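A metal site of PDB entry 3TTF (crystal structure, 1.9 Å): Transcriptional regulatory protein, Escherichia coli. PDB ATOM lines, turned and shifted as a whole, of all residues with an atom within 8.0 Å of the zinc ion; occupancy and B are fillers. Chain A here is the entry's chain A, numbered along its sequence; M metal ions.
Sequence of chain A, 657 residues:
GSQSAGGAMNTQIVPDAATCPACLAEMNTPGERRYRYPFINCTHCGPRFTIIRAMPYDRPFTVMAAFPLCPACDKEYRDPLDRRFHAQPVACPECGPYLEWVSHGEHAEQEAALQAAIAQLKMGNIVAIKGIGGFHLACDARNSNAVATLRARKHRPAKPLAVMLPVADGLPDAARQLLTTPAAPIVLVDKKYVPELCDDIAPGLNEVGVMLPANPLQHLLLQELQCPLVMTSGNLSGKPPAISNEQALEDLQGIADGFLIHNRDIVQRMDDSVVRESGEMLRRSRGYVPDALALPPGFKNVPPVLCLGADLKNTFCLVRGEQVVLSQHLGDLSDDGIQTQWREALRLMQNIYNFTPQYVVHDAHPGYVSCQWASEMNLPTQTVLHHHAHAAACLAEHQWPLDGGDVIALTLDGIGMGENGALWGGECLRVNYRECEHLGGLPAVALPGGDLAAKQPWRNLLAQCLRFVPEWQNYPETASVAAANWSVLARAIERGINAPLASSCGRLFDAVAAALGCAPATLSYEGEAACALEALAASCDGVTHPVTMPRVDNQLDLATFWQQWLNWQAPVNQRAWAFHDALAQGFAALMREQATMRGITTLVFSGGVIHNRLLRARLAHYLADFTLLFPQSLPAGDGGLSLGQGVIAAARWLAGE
The side-chain sulfur (SG) of Cys 23 sits close to the guanidinium group (NH2) of Arg 83 (3.5 Å). The side-chain sulfur of Cys 23 lies close to the guanidinium group of Arg 84 (3.5 Å). The side-chain amide nitrogen of Asn 41 sits at hydrogen-bond distance from the backbone carbonyl oxygen of Cys 45 (3.4 Å). The guanidinium group of Arg 48 lies within hydrogen-bond range of the backbone carbonyl oxygen of Cys 45, 2.9 Å away. The side-chain sulfur (SG) of Cys 42 sits close to the guanidinium group (NE) of Arg 83, 3.6 Å away. N of His 44 lies close to SG of Cys 42 (3.4 Å). The guanidinium group (NH1) of Arg 48 sits at hydrogen-bond distance from the backbone carbonyl oxygen (O) of Cys 42 (2.9 Å).
Within 4 Å of the zinc ion: Cys 20, Cys 23, Cys 42 and Cys 45.
The zinc ion is bound by SG of Cys 20 (2.3 Å), SG of Cys 23 (2.3 Å), SG of Cys 45 (2.4 Å) and SG of Cys 42 (2.5 Å).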
ATOM      1  N   ALA A  17      24.121  -4.817   0.856  1.00  0.00           N
ATOM      2  CA  ALA A  17      22.862  -4.233   0.360  1.00  0.00           C
ATOM      3  C   ALA A  17      21.670  -4.391   1.315  1.00  0.00           C
ATOM      4  O   ALA A  17      21.529  -5.415   1.988  1.00  0.00           O
ATOM      5  CB  ALA A  17      22.504  -4.781  -1.038  1.00  0.00           C
ATOM      6  N   ALA A  18      20.810  -3.367   1.369  1.00  0.00           N
ATOM      7  CA  ALA A  18      19.655  -3.361   2.290  1.00  0.00           C
ATOM      8  C   ALA A  18      18.748  -4.559   2.053  1.00  0.00           C
ATOM      9  O   ALA A  18      18.478  -4.918   0.914  1.00  0.00           O
ATOM     10  CB  ALA A  18      18.859  -2.080   2.122  1.00  0.00           C
ATOM     11  N   THR A  19      18.292  -5.177   3.146  1.00  0.00           N
ATOM     12  CA  THR A  19      17.300  -6.239   3.078  1.00  0.00           C
ATOM     13  C   THR A  19      16.177  -5.964   2.049  1.00  0.00           C
ATOM     14  O   THR A  19      15.518  -4.931   2.125  1.00  0.00           O
ATOM     15  CB  THR A  19      16.735  -6.539   4.485  1.00  0.00           C
ATOM     16  OG1 THR A  19      17.822  -6.943   5.309  1.00  0.00           O
ATOM     17  CG2 THR A  19      15.715  -7.667   4.460  1.00  0.00           C
ATOM     18  N   CYS A  20      15.983  -6.895   1.103  1.00  0.00           N
ATOM     19  CA  CYS A  20      14.981  -6.769   0.019  1.00  0.00           C
ATOM     20  C   CYS A  20      13.534  -7.015   0.475  1.00  0.00           C
ATOM     21  O   CYS A  20      13.314  -7.670   1.500  1.00  0.00           O
ATOM     22  CB  CYS A  20      15.339  -7.680  -1.182  1.00  0.00           C
ATOM     23  SG  CYS A  20      15.068  -9.529  -1.021  1.00  0.00           S
ATOM     24  N   PRO A  21      12.550  -6.493  -0.262  1.00  0.00           N
ATOM     25  CA  PRO A  21      11.150  -6.688   0.122  1.00  0.00           C
ATOM     26  C   PRO A  21      10.748  -8.167   0.262  1.00  0.00           C
ATOM     27  O   PRO A  21       9.957  -8.505   1.135  1.00  0.00           O
ATOM     28  CB  PRO A  21      10.359  -6.020  -1.017  1.00  0.00           C
ATOM     29  CG  PRO A  21      11.316  -5.024  -1.600  1.00  0.00           C
ATOM     30  CD  PRO A  21      12.671  -5.663  -1.468  1.00  0.00           C
ATOM     31  N   ALA A  22      11.318  -9.036  -0.588  1.00  0.00           N
ATOM     32  CA  ALA A  22      11.080 -10.474  -0.526  1.00  0.00           C
ATOM     33  C   ALA A  22      11.522 -11.084   0.814  1.00  0.00           C
ATOM     34  O   ALA A  22      10.756 -11.829   1.430  1.00  0.00           O
ATOM     35  CB  ALA A  22      11.780 -11.164  -1.681  1.00  0.00           C
ATOM     36  N   CYS A  23      12.752 -10.781   1.245  1.00  0.00           N
ATOM     37  CA  CYS A  23      13.255 -11.228   2.532  1.00  0.00           C
ATOM     38  C   CYS A  23      12.480 -10.617   3.701  1.00  0.00           C
ATOM     39  O   CYS A  23      12.208 -11.300   4.686  1.00  0.00           O
ATOM     40  CB  CYS A  23      14.749 -10.940   2.677  1.00  0.00           C
ATOM     41  SG  CYS A  23      15.790 -12.016   1.644  1.00  0.00           S
ATOM     42  N   LEU A  24      12.116  -9.354   3.585  1.00  0.00           N
ATOM     43  CA  LEU A  24      11.279  -8.709   4.598  1.00  0.00           C
ATOM     44  C   LEU A  24       9.923  -9.415   4.760  1.00  0.00           C
ATOM     45  O   LEU A  24       9.482  -9.616   5.887  1.00  0.00           O
ATOM     46  CB  LEU A  24      11.130  -7.203   4.338  1.00  0.00           C
ATOM     47  CG  LEU A  24      10.567  -6.323   5.462  1.00  0.00           C
ATOM     48  CD1 LEU A  24      11.277  -6.599   6.779  1.00  0.00           C
ATOM     49  CD2 LEU A  24      10.611  -4.827   5.109  1.00  0.00           C
ATOM     50  N   GLU A  26       9.237 -12.676   3.988  1.00  0.00           N
ATOM     51  CA  GLU A  26       9.512 -13.998   4.537  1.00  0.00           C
ATOM     52  C   GLU A  26       9.728 -13.947   6.057  1.00  0.00           C
ATOM     53  O   GLU A  26       9.162 -14.765   6.802  1.00  0.00           O
ATOM     54  CB  GLU A  26      10.717 -14.629   3.852  1.00  0.00           C
ATOM     55  CG  GLU A  26      10.957 -16.094   4.205  1.00  0.00           C
ATOM     56  CD  GLU A  26      12.070 -16.717   3.371  1.00  0.00           C
ATOM     57  OE1 GLU A  26      12.343 -16.188   2.262  1.00  0.00           O
ATOM     58  OE2 GLU A  26      12.674 -17.713   3.834  1.00  0.00           O
ATOM     59  N   ILE A  40      18.261 -13.346   7.894  1.00  0.00           N
ATOM     60  CA  ILE A  40      17.728 -13.664   6.579  1.00  0.00           C
ATOM     61  C   ILE A  40      18.353 -12.744   5.511  1.00  0.00           C
ATOM     62  O   ILE A  40      18.553 -11.543   5.749  1.00  0.00           O
ATOM     63  CB  ILE A  40      16.190 -13.573   6.544  1.00  0.00           C
ATOM     64  CG1 ILE A  40      15.637 -14.042   5.196  1.00  0.00           C
ATOM     65  CG2 ILE A  40      15.713 -12.167   6.881  1.00  0.00           C
ATOM     66  CD1 ILE A  40      14.157 -14.310   5.206  1.00  0.00           C
ATOM     67  N   ASN A  41      18.700 -13.338   4.372  1.00  0.00           N
ATOM     68  CA  ASN A  41      19.148 -12.626   3.188  1.00  0.00           C
ATOM     69  C   ASN A  41      19.031 -13.589   2.024  1.00  0.00           C
ATOM     70  O   ASN A  41      18.668 -14.749   2.222  1.00  0.00           O
ATOM     71  CB  ASN A  41      20.584 -12.105   3.337  1.00  0.00           C
ATOM     72  CG  ASN A  41      21.625 -13.216   3.259  1.00  0.00           C
ATOM     73  OD1 ASN A  41      21.752 -14.028   4.168  1.00  0.00           O
ATOM     74  ND2 ASN A  41      22.405 -13.235   2.169  1.00  0.00           N
ATOM     75  N   CYS A  42      19.307 -13.101   0.814  1.00  0.00           N
ATOM     76  CA  CYS A  42      19.300 -13.935  -0.379  1.00  0.00           C
ATOM     77  C   CYS A  42      20.244 -13.348  -1.407  1.00  0.00           C
ATOM     78  O   CYS A  42      21.145 -12.593  -1.073  1.00  0.00           O
ATOM     79  CB  CYS A  42      17.880 -13.994  -0.943  1.00  0.00           C
ATOM     80  SG  CYS A  42      17.400 -12.407  -1.606  1.00  0.00           S
ATOM     81  N   THR A  43      19.992 -13.668  -2.684  1.00  0.00           N
ATOM     82  CA  THR A  43      20.838 -13.249  -3.796  1.00  0.00           C
ATOM     83  C   THR A  43      20.850 -11.733  -4.021  1.00  0.00           C
ATOM     84  O   THR A  43      21.868 -11.184  -4.465  1.00  0.00           O
ATOM     85  CB  THR A  43      20.425 -13.992  -5.115  1.00  0.00           C
ATOM     86  OG1 THR A  43      20.580 -15.414  -4.920  1.00  0.00           O
ATOM     87  CG2 THR A  43      21.276 -13.552  -6.310  1.00  0.00           C
ATOM     88  N   HIS A  44      19.747 -11.059  -3.701  1.00  0.00           N
ATOM     89  CA  HIS A  44      19.624  -9.617  -3.987  1.00  0.00           C
ATOM     90  C   HIS A  44      19.901  -8.693  -2.805  1.00  0.00           C
ATOM     91  O   HIS A  44      19.819  -7.466  -2.961  1.00  0.00           O
ATOM     92  CB  HIS A  44      18.256  -9.320  -4.599  1.00  0.00           C
ATOM     93  CG  HIS A  44      17.963 -10.140  -5.807  1.00  0.00           C
ATOM     94  ND1 HIS A  44      17.062 -11.182  -5.806  1.00  0.00           N
ATOM     95  CD2 HIS A  44      18.489 -10.093  -7.053  1.00  0.00           C
ATOM     96  CE1 HIS A  44      17.044 -11.745  -6.996  1.00  0.00           C
ATOM     97  NE2 HIS A  44      17.899 -11.107  -7.779  1.00  0.00           N
ATOM     98  N   CYS A  45      20.234  -9.269  -1.649  1.00  0.00           N
ATOM     99  CA  CYS A  45      20.407  -8.480  -0.439  1.00  0.00           C
ATOM    100  C   CYS A  45      21.287  -9.188   0.572  1.00  0.00           C
ATOM    101  O   CYS A  45      21.536 -10.392   0.458  1.00  0.00           O
ATOM    102  CB  CYS A  45      19.052  -8.137   0.185  1.00  0.00           C
ATOM    103  SG  CYS A  45      18.372  -9.363   1.307  1.00  0.00           S
ATOM    104  N   GLY A  46      21.768  -8.406   1.537  1.00  0.00           N
ATOM    105  CA  GLY A  46      22.518  -8.935   2.685  1.00  0.00           C
ATOM    106  C   GLY A  46      23.950  -8.448   2.663  1.00  0.00           C
ATOM    107  O   GLY A  46      24.300  -7.636   1.826  1.00  0.00           O
ATOM    108  N   ARG A  48      27.959  -8.369   2.017  1.00  0.00           N
ATOM    109  CA  ARG A  48      28.854  -8.912   0.997  1.00  0.00           C
ATOM    110  C   ARG A  48      30.285  -8.666   1.443  1.00  0.00           C
ATOM    111  O   ARG A  48      30.912  -9.509   2.085  1.00  0.00           O
ATOM    112  CB  ARG A  48      28.590  -8.266  -0.373  1.00  0.00           C
ATOM    113  CG  ARG A  48      27.146  -8.353  -0.911  1.00  0.00           C
ATOM    114  CD  ARG A  48      26.572  -9.766  -0.857  1.00  0.00           C
ATOM    115  NE  ARG A  48      25.281  -9.876  -1.541  1.00  0.00           N
ATOM    116  CZ  ARG A  48      24.299 -10.723  -1.228  1.00  0.00           C
ATOM    117  NH1 ARG A  48      23.178 -10.711  -1.940  1.00  0.00           N
ATOM    118  NH2 ARG A  48      24.406 -11.565  -0.212  1.00  0.00           N
ATOM    119  N   ARG A  83      14.927 -18.300  -5.041  1.00  0.00           N
ATOM    120  CA  ARG A  83      15.564 -16.980  -4.926  1.00  0.00           C
ATOM    121  C   ARG A  83      16.892 -17.088  -4.153  1.00  0.00           C
ATOM    122  O   ARG A  83      17.569 -16.075  -3.918  1.00  0.00           O
ATOM    123  CB  ARG A  83      14.595 -16.017  -4.224  1.00  0.00           C
ATOM    124  CG  ARG A  83      14.937 -14.527  -4.345  1.00  0.00           C
ATOM    125  CD  ARG A  83      13.885 -13.664  -3.628  1.00  0.00           C
ATOM    126  NE  ARG A  83      14.067 -13.604  -2.170  1.00  0.00           N
ATOM    127  CZ  ARG A  83      13.372 -14.323  -1.288  1.00  0.00           C
ATOM    128  NH1 ARG A  83      12.434 -15.175  -1.696  1.00  0.00           N
ATOM    129  NH2 ARG A  83      13.606 -14.189   0.015  1.00  0.00           N
ATOM    130  N   ARG A  84      17.238 -18.317  -3.774  1.00  0.00           N
ATOM    131  CA  ARG A  84      18.429 -18.580  -2.955  1.00  0.00           C
ATOM    132  C   ARG A  84      19.459 -19.510  -3.609  1.00  0.00           C
ATOM    133  O   ARG A  84      20.323 -20.074  -2.913  1.00  0.00           O
ATOM    134  CB  ARG A  84      18.022 -19.078  -1.568  1.00  0.00           C
ATOM    135  CG  ARG A  84      17.238 -18.066  -0.812  1.00  0.00           C
ATOM    136  CD  ARG A  84      17.286 -18.309   0.662  1.00  0.00           C
ATOM    137  NE  ARG A  84      16.991 -17.091   1.395  1.00  0.00           N
ATOM    138  CZ  ARG A  84      15.770 -16.601   1.593  1.00  0.00           C
ATOM    139  NH1 ARG A  84      14.698 -17.228   1.116  1.00  0.00           N
ATOM    140  NH2 ARG A  84      15.622 -15.471   2.268  1.00  0.00           N
HETATM  141 ZN    ZN M   1      16.766 -10.635   0.067  1.00  0.00          ZN
